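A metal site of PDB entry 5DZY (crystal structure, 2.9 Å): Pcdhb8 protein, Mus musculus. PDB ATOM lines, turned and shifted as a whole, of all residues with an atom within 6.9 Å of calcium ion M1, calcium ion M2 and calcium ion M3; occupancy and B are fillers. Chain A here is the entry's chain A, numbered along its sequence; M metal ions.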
ATOM      1  N   GLU A 225     -24.360   4.152   9.572  1.00  0.00           N
ATOM      2  CA  GLU A 225     -25.051   2.979   9.045  1.00  0.00           C
ATOM      3  C   GLU A 225     -26.299   3.373   8.261  1.00  0.00           C
ATOM      4  O   GLU A 225     -26.644   2.747   7.259  1.00  0.00           O
ATOM      5  CB  GLU A 225     -25.425   2.030  10.171  1.00  0.00           C
ATOM      6  CG  GLU A 225     -26.209   0.800   9.738  1.00  0.00           C
ATOM      7  CD  GLU A 225     -26.590  -0.097  10.900  1.00  0.00           C
ATOM      8  OE1 GLU A 225     -26.164   0.199  12.046  1.00  0.00           O
ATOM      9  OE2 GLU A 225     -27.299  -1.092  10.676  1.00  0.00           O
ATOM     10  N   LEU A 278     -25.761  -0.615   4.223  1.00  0.00           N
ATOM     11  CA  LEU A 278     -24.765  -0.784   5.271  1.00  0.00           C
ATOM     12  C   LEU A 278     -25.410  -1.219   6.585  1.00  0.00           C
ATOM     13  O   LEU A 278     -26.508  -0.783   6.916  1.00  0.00           O
ATOM     14  CB  LEU A 278     -23.972   0.507   5.497  1.00  0.00           C
ATOM     15  CG  LEU A 278     -22.769   0.741   4.576  1.00  0.00           C
ATOM     16  CD1 LEU A 278     -22.065   2.035   4.946  1.00  0.00           C
ATOM     17  CD2 LEU A 278     -21.813  -0.438   4.649  1.00  0.00           C
ATOM     18  N   ASP A 279     -24.721  -2.101   7.303  1.00  0.00           N
ATOM     19  CA  ASP A 279     -25.208  -2.558   8.609  1.00  0.00           C
ATOM     20  C   ASP A 279     -24.039  -2.786   9.556  1.00  0.00           C
ATOM     21  O   ASP A 279     -23.196  -3.658   9.326  1.00  0.00           O
ATOM     22  CB  ASP A 279     -26.025  -3.845   8.457  1.00  0.00           C
ATOM     23  CG  ASP A 279     -26.723  -4.238   9.738  1.00  0.00           C
ATOM     24  OD1 ASP A 279     -27.876  -3.810   9.937  1.00  0.00           O
ATOM     25  OD2 ASP A 279     -26.121  -4.986  10.545  1.00  0.00           O
ATOM     26  N   PHE A 280     -24.000  -1.997  10.632  1.00  0.00           N
ATOM     27  CA  PHE A 280     -22.924  -2.071  11.607  1.00  0.00           C
ATOM     28  C   PHE A 280     -22.872  -3.424  12.304  1.00  0.00           C
ATOM     29  O   PHE A 280     -21.818  -3.864  12.755  1.00  0.00           O
ATOM     30  CB  PHE A 280     -23.082  -0.948  12.634  1.00  0.00           C
ATOM     31  CG  PHE A 280     -22.005  -0.916  13.679  1.00  0.00           C
ATOM     32  CD1 PHE A 280     -20.795  -0.292  13.436  1.00  0.00           C
ATOM     33  CD2 PHE A 280     -22.199  -1.510  14.921  1.00  0.00           C
ATOM     34  CE1 PHE A 280     -19.800  -0.259  14.395  1.00  0.00           C
ATOM     35  CE2 PHE A 280     -21.209  -1.483  15.887  1.00  0.00           C
ATOM     36  CZ  PHE A 280     -20.013  -0.853  15.625  1.00  0.00           C
ATOM     37  N   GLU A 281     -24.027  -4.087  12.380  1.00  0.00           N
ATOM     38  CA  GLU A 281     -24.134  -5.361  13.072  1.00  0.00           C
ATOM     39  C   GLU A 281     -23.649  -6.514  12.193  1.00  0.00           C
ATOM     40  O   GLU A 281     -23.283  -7.576  12.701  1.00  0.00           O
ATOM     41  CB  GLU A 281     -25.579  -5.613  13.517  1.00  0.00           C
ATOM     42  CG  GLU A 281     -26.036  -4.743  14.673  1.00  0.00           C
ATOM     43  CD  GLU A 281     -26.149  -3.282  14.309  1.00  0.00           C
ATOM     44  OE1 GLU A 281     -26.582  -2.989  13.173  1.00  0.00           O
ATOM     45  OE2 GLU A 281     -25.802  -2.423  15.147  1.00  0.00           O
ATOM     46  N   ALA A 282     -23.650  -6.311  10.881  1.00  0.00           N
ATOM     47  CA  ALA A 282     -23.154  -7.312   9.956  1.00  0.00           C
ATOM     48  C   ALA A 282     -21.652  -7.133   9.726  1.00  0.00           C
ATOM     49  O   ALA A 282     -20.862  -8.023  10.041  1.00  0.00           O
ATOM     50  CB  ALA A 282     -23.900  -7.235   8.633  1.00  0.00           C
ATOM     51  N   LEU A 309     -20.466   3.598  11.390  1.00  0.00           N
ATOM     52  CA  LEU A 309     -20.963   4.064  12.677  1.00  0.00           C
ATOM     53  C   LEU A 309     -22.240   3.318  13.053  1.00  0.00           C
ATOM     54  O   LEU A 309     -23.062   3.001  12.194  1.00  0.00           O
ATOM     55  CB  LEU A 309     -21.219   5.563  12.651  1.00  0.00           C
ATOM     56  CG  LEU A 309     -20.006   6.468  12.401  1.00  0.00           C
ATOM     57  CD1 LEU A 309     -20.432   7.927  12.384  1.00  0.00           C
ATOM     58  CD2 LEU A 309     -18.932   6.218  13.453  1.00  0.00           C
ATOM     59  N   ASP A 310     -22.401   3.033  14.346  1.00  0.00           N
ATOM     60  CA  ASP A 310     -23.567   2.307  14.830  1.00  0.00           C
ATOM     61  C   ASP A 310     -24.788   3.224  14.946  1.00  0.00           C
ATOM     62  O   ASP A 310     -24.693   4.348  15.438  1.00  0.00           O
ATOM     63  CB  ASP A 310     -23.278   1.652  16.175  1.00  0.00           C
ATOM     64  CG  ASP A 310     -24.477   0.897  16.729  1.00  0.00           C
ATOM     65  OD1 ASP A 310     -25.251   0.345  15.923  1.00  0.00           O
ATOM     66  OD2 ASP A 310     -24.635   0.852  17.966  1.00  0.00           O
ATOM     67  N   VAL A 311     -25.931   2.728  14.492  1.00  0.00           N
ATOM     68  CA  VAL A 311     -27.195   3.432  14.628  1.00  0.00           C
ATOM     69  C   VAL A 311     -28.214   2.536  15.328  1.00  0.00           C
ATOM     70  O   VAL A 311     -28.366   1.377  14.973  1.00  0.00           O
ATOM     71  CB  VAL A 311     -27.758   3.885  13.266  1.00  0.00           C
ATOM     72  CG1 VAL A 311     -29.060   4.656  13.442  1.00  0.00           C
ATOM     73  CG2 VAL A 311     -26.726   4.734  12.522  1.00  0.00           C
ATOM     74  N   ASN A 312     -28.902   3.082  16.327  1.00  0.00           N
ATOM     75  CA  ASN A 312     -29.902   2.316  17.056  1.00  0.00           C
ATOM     76  C   ASN A 312     -31.102   1.987  16.184  1.00  0.00           C
ATOM     77  O   ASN A 312     -32.132   2.668  16.233  1.00  0.00           O
ATOM     78  CB  ASN A 312     -30.348   3.072  18.304  1.00  0.00           C
ATOM     79  CG  ASN A 312     -31.198   2.222  19.232  1.00  0.00           C
ATOM     80  OD1 ASN A 312     -31.147   0.989  19.180  1.00  0.00           O
ATOM     81  ND2 ASN A 312     -31.963   2.874  20.100  1.00  0.00           N
ATOM     82  N   ASP A 313     -30.977   0.940  15.369  1.00  0.00           N
ATOM     83  CA  ASP A 313     -32.040   0.548  14.457  1.00  0.00           C
ATOM     84  C   ASP A 313     -32.535  -0.870  14.747  1.00  0.00           C
ATOM     85  O   ASP A 313     -33.217  -1.486  13.925  1.00  0.00           O
ATOM     86  CB  ASP A 313     -31.566   0.652  13.007  1.00  0.00           C
ATOM     87  CG  ASP A 313     -30.388  -0.264  12.702  1.00  0.00           C
ATOM     88  OD1 ASP A 313     -29.705  -0.694  13.656  1.00  0.00           O
ATOM     89  OD2 ASP A 313     -30.150  -0.545  11.509  1.00  0.00           O
ATOM     90  N   ASN A 314     -32.176  -1.394  15.925  1.00  0.00           N
ATOM     91  CA  ASN A 314     -32.613  -2.719  16.330  1.00  0.00           C
ATOM     92  C   ASN A 314     -33.337  -2.721  17.669  1.00  0.00           C
ATOM     93  O   ASN A 314     -32.827  -2.192  18.667  1.00  0.00           O
ATOM     94  CB  ASN A 314     -31.422  -3.683  16.389  1.00  0.00           C
ATOM     95  CG  ASN A 314     -30.988  -4.159  15.020  1.00  0.00           C
ATOM     96  OD1 ASN A 314     -29.832  -4.004  14.629  1.00  0.00           O
ATOM     97  ND2 ASN A 314     -31.916  -4.748  14.278  1.00  0.00           N
ATOM     98  N   ALA A 315     -34.519  -3.317  17.692  1.00  0.00           N
ATOM     99  CA  ALA A 315     -35.284  -3.466  18.930  1.00  0.00           C
ATOM    100  C   ALA A 315     -34.826  -4.710  19.679  1.00  0.00           C
ATOM    101  O   ALA A 315     -34.435  -5.704  19.064  1.00  0.00           O
ATOM    102  CB  ALA A 315     -36.775  -3.533  18.630  1.00  0.00           C
ATOM    103  N   PRO A 316     -34.857  -4.656  21.026  1.00  0.00           N
ATOM    104  CA  PRO A 316     -34.472  -5.805  21.857  1.00  0.00           C
ATOM    105  C   PRO A 316     -35.302  -7.050  21.569  1.00  0.00           C
ATOM    106  O   PRO A 316     -36.519  -6.952  21.417  1.00  0.00           O
ATOM    107  CB  PRO A 316     -34.724  -5.305  23.286  1.00  0.00           C
ATOM    108  CG  PRO A 316     -34.635  -3.818  23.187  1.00  0.00           C
ATOM    109  CD  PRO A 316     -35.187  -3.477  21.832  1.00  0.00           C
ATOM    110  N   SER A 342     -32.012 -10.075  23.976  1.00  0.00           N
ATOM    111  CA  SER A 342     -30.929  -9.960  23.007  1.00  0.00           C
ATOM    112  C   SER A 342     -30.886  -8.579  22.370  1.00  0.00           C
ATOM    113  O   SER A 342     -31.890  -7.880  22.305  1.00  0.00           O
ATOM    114  CB  SER A 342     -31.057 -11.038  21.930  1.00  0.00           C
ATOM    115  OG  SER A 342     -30.018 -10.938  20.978  1.00  0.00           O
ATOM    116  N   ASP A 343     -29.706  -8.187  21.893  1.00  0.00           N
ATOM    117  CA  ASP A 343     -29.522  -6.915  21.208  1.00  0.00           C
ATOM    118  C   ASP A 343     -28.218  -6.914  20.421  1.00  0.00           C
ATOM    119  O   ASP A 343     -27.139  -6.949  21.007  1.00  0.00           O
ATOM    120  CB  ASP A 343     -29.541  -5.748  22.208  1.00  0.00           C
ATOM    121  CG  ASP A 343     -29.809  -4.414  21.548  1.00  0.00           C
ATOM    122  OD1 ASP A 343     -29.519  -4.263  20.342  1.00  0.00           O
ATOM    123  OD2 ASP A 343     -30.308  -3.502  22.241  1.00  0.00           O
ATOM    124  N   PRO A 344     -28.318  -6.856  19.086  1.00  0.00           N
ATOM    125  CA  PRO A 344     -27.147  -6.882  18.199  1.00  0.00           C
ATOM    126  C   PRO A 344     -26.385  -5.558  18.196  1.00  0.00           C
ATOM    127  O   PRO A 344     -25.234  -5.517  17.756  1.00  0.00           O
ATOM    128  CB  PRO A 344     -27.752  -7.167  16.833  1.00  0.00           C
ATOM    129  CG  PRO A 344     -29.119  -6.591  16.911  1.00  0.00           C
ATOM    130  CD  PRO A 344     -29.574  -6.817  18.322  1.00  0.00           C
ATOM    131  N   ASP A 345     -27.019  -4.492  18.669  1.00  0.00           N
ATOM    132  CA  ASP A 345     -26.394  -3.171  18.698  1.00  0.00           C
ATOM    133  C   ASP A 345     -25.247  -3.111  19.698  1.00  0.00           C
ATOM    134  O   ASP A 345     -25.026  -4.042  20.470  1.00  0.00           O
ATOM    135  CB  ASP A 345     -27.434  -2.090  19.028  1.00  0.00           C
ATOM    136  CG  ASP A 345     -28.543  -2.019  17.998  1.00  0.00           C
ATOM    137  OD1 ASP A 345     -28.294  -2.346  16.821  1.00  0.00           O
ATOM    138  OD2 ASP A 345     -29.673  -1.633  18.369  1.00  0.00           O
ATOM    139  N   SER A 346     -24.508  -2.001  19.670  1.00  0.00           N
ATOM    140  CA  SER A 346     -23.368  -1.820  20.571  1.00  0.00           C
ATOM    141  C   SER A 346     -23.555  -0.605  21.476  1.00  0.00           C
ATOM    142  O   SER A 346     -24.391   0.251  21.203  1.00  0.00           O
ATOM    143  CB  SER A 346     -22.078  -1.682  19.767  1.00  0.00           C
ATOM    144  OG  SER A 346     -22.126  -0.547  18.913  1.00  0.00           O
ATOM    145  N   ASP A 348     -24.691   1.764  24.494  1.00  0.00           N
ATOM    146  CA  ASP A 348     -25.974   1.905  25.189  1.00  0.00           C
ATOM    147  C   ASP A 348     -27.117   1.442  24.296  1.00  0.00           C
ATOM    148  O   ASP A 348     -28.204   1.127  24.782  1.00  0.00           O
ATOM    149  CB  ASP A 348     -26.186   3.351  25.618  1.00  0.00           C
ATOM    150  CG  ASP A 348     -25.189   3.806  26.666  1.00  0.00           C
ATOM    151  OD1 ASP A 348     -24.569   2.932  27.313  1.00  0.00           O
ATOM    152  OD2 ASP A 348     -25.020   5.026  26.849  1.00  0.00           O
ATOM    153  N   ASN A 349     -26.874   1.400  22.990  1.00  0.00           N
ATOM    154  CA  ASN A 349     -27.854   0.888  22.041  1.00  0.00           C
ATOM    155  C   ASN A 349     -28.023  -0.616  22.216  1.00  0.00           C
ATOM    156  O   ASN A 349     -29.070  -1.176  21.895  1.00  0.00           O
ATOM    157  CB  ASN A 349     -27.438   1.204  20.602  1.00  0.00           C
ATOM    158  CG  ASN A 349     -27.242   2.689  20.373  1.00  0.00           C
ATOM    159  OD1 ASN A 349     -27.859   3.523  21.023  1.00  0.00           O
ATOM    160  ND2 ASN A 349     -26.363   3.022  19.434  1.00  0.00           N
ATOM    161  N   GLY A 350     -26.985  -1.269  22.734  1.00  0.00           N
ATOM    162  CA  GLY A 350     -27.011  -2.693  22.986  1.00  0.00           C
ATOM    163  C   GLY A 350     -27.385  -3.014  24.421  1.00  0.00           C
ATOM    164  O   GLY A 350     -27.936  -4.080  24.703  1.00  0.00           O
ATOM    165  N   ARG A 351     -27.097  -2.087  25.329  1.00  0.00           N
ATOM    166  CA  ARG A 351     -27.454  -2.241  26.734  1.00  0.00           C
ATOM    167  C   ARG A 351     -28.960  -2.106  26.904  1.00  0.00           C
ATOM    168  O   ARG A 351     -29.572  -1.221  26.301  1.00  0.00           O
ATOM    169  CB  ARG A 351     -26.718  -1.230  27.601  1.00  0.00           C
ATOM    170  CG  ARG A 351     -26.995  -1.371  29.087  1.00  0.00           C
ATOM    171  CD  ARG A 351     -26.106  -0.463  29.922  1.00  0.00           C
ATOM    172  NE  ARG A 351     -24.687  -0.758  29.724  1.00  0.00           N
ATOM    173  CZ  ARG A 351     -23.806   0.108  29.253  1.00  0.00           C
ATOM    174  NH1 ARG A 351     -24.191   1.341  28.940  1.00  0.00           N
ATOM    175  NH2 ARG A 351     -22.529  -0.238  29.104  1.00  0.00           N
ATOM    176  N   ASP A 396     -34.034  -0.651  25.597  1.00  0.00           N
ATOM    177  CA  ASP A 396     -32.624  -0.291  25.533  1.00  0.00           C
ATOM    178  C   ASP A 396     -32.358   1.087  26.143  1.00  0.00           C
ATOM    179  O   ASP A 396     -33.292   1.847  26.409  1.00  0.00           O
ATOM    180  CB  ASP A 396     -32.119  -0.322  24.086  1.00  0.00           C
ATOM    181  CG  ASP A 396     -33.034   0.417  23.125  1.00  0.00           C
ATOM    182  OD1 ASP A 396     -33.709   1.380  23.545  1.00  0.00           O
ATOM    183  OD2 ASP A 396     -33.083   0.026  21.935  1.00  0.00           O
ATOM    184  N   LEU A 397     -31.094   1.403  26.350  1.00  0.00           N
ATOM    185  CA  LEU A 397     -30.707   2.695  26.917  1.00  0.00           C
ATOM    186  C   LEU A 397     -30.062   3.594  25.869  1.00  0.00           C
ATOM    187  O   LEU A 397     -29.246   4.460  26.197  1.00  0.00           O
ATOM    188  CB  LEU A 397     -29.739   2.490  28.091  1.00  0.00           C
ATOM    189  CG  LEU A 397     -30.293   1.741  29.308  1.00  0.00           C
ATOM    190  CD1 LEU A 397     -29.214   1.573  30.371  1.00  0.00           C
ATOM    191  CD2 LEU A 397     -31.504   2.459  29.871  1.00  0.00           C
ATOM    192  N   GLY A 398     -30.434   3.380  24.607  1.00  0.00           N
ATOM    193  CA  GLY A 398     -29.873   4.150  23.514  1.00  0.00           C
ATOM    194  C   GLY A 398     -30.702   5.373  23.157  1.00  0.00           C
ATOM    195  O   GLY A 398     -31.728   5.639  23.783  1.00  0.00           O
ATOM    196  N   PRO A 400     -32.378   7.216  19.695  1.00  0.00           N
ATOM    197  CA  PRO A 400     -33.617   7.138  20.482  1.00  0.00           C
ATOM    198  C   PRO A 400     -33.818   5.777  21.142  1.00  0.00           C
ATOM    199  O   PRO A 400     -33.174   4.795  20.757  1.00  0.00           O
ATOM    200  CB  PRO A 400     -34.720   7.388  19.439  1.00  0.00           C
ATOM    201  CG  PRO A 400     -34.021   7.975  18.254  1.00  0.00           C
ATOM    202  CD  PRO A 400     -32.662   7.352  18.249  1.00  0.00           C
ATOM    203  N   LEU A 402     -35.630   2.327  22.100  1.00  0.00           N
ATOM    204  CA  LEU A 402     -36.536   1.356  21.509  1.00  0.00           C
ATOM    205  C   LEU A 402     -37.057   0.375  22.565  1.00  0.00           C
ATOM    206  O   LEU A 402     -36.289  -0.164  23.363  1.00  0.00           O
ATOM    207  CB  LEU A 402     -35.848   0.582  20.389  1.00  0.00           C
ATOM    208  CG  LEU A 402     -35.374   1.394  19.179  1.00  0.00           C
ATOM    209  CD1 LEU A 402     -34.690   0.502  18.167  1.00  0.00           C
ATOM    210  CD2 LEU A 402     -36.545   2.130  18.547  1.00  0.00           C
HETATM  211 CA    CA M   1     -31.041  -1.495  20.402  1.00  0.00          CA
HETATM  212 CA    CA M   2     -27.316  -0.835  14.700  1.00  0.00          CA
HETATM  213 CA    CA M   3     -28.611  -2.412  11.869  1.00  0.00          CA
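The side-chain carboxylate (OE1) of Glu 225 sits close to the backbone NH (N) of Phe 280 (3.4 Å).
The backbone NH of Glu 225 sits at hydrogen-bond distance from the backbone carbonyl oxygen of Leu 309, 3.1 Å away.
The side-chain amide oxygen (OD1) of Asn 314 sits close to the side-chain carboxylate (OD1) of Asp 313, 3.5 Å away.
ND2 of Asn 349 sits at hydrogen-bond distance from OD2 of Asp 310, 3.1 Å away.
N of Ala 282 lies within hydrogen-bond range of OD2 of Asp 279, at 2.8 Å.
OD2 of Asp 310 is in hydrogen-bond range of OG of Ser 346 (3.0 Å).
OD1 of Asp 396 sits at hydrogen-bond distance from N of Leu 402 (2.6 Å).
Six residues have an atom within 4 Å of calcium ion M1: Asn 312, Asn 314, Asp 343, Asp 345, Asn 349 and Asp 396.
Along chain A the residues within 4 Å of calcium ion M1 span positions 312 to 396.
Of the 28 residues printed, 6 come within 4 Å of calcium ion M2.
The nearest printed residue that does not touch calcium ion M2 is Asn 314 (4.05 Å).
Within 4 Å of calcium ion M3: Glu 225, Asp 279, Glu 281, Asp 313 and Asn 314.
OD2 of Asp 345 binds calcium ion M1.
The backbone carbonyl oxygen (O) of Asn 349 binds calcium ion M1.
O of Asn 314 binds calcium ion M1.
Calcium ion M1 is bound by OD1 of Asn 312 (2.8 Å).
Calcium ion M1 is bound by OD2 of Asp 343, 2.8 Å away.
Calcium ion M1 has five donor atoms within binding distance.
Slightly farther from calcium ion M1 lies the side-chain carboxylate (OD2) of Asp 396 (3.0 Å).
Calcium ion M2 is bound by the side-chain carboxylate (OE2) of Glu 281, the backbone carbonyl oxygen (O) of Val 311, the side-chain carboxylate (OD1) of Asp 313, the side-chain carboxylate (OD1) of Asp 310, the side-chain carboxylate (OE1) of Glu 281 and the side-chain carboxylate (OD1) of Asp 345.
Slightly farther from calcium ion M2 lies the side-chain carboxylate (OE1) of Glu 225 (3.1 Å).
Calcium ion M3 is bound by the side-chain carboxylate (OE2) of Glu 225 (2.2 Å), the side-chain carboxylate (OD2) of Asp 313 (2.4 Å), the side-chain carboxylate (OE1) of Glu 281 (2.5 Å), the side-chain carboxylate (OD1) of Asp 279 (2.5 Å) and the side-chain carboxylate (OD1) of Asp 313 (2.7 Å).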
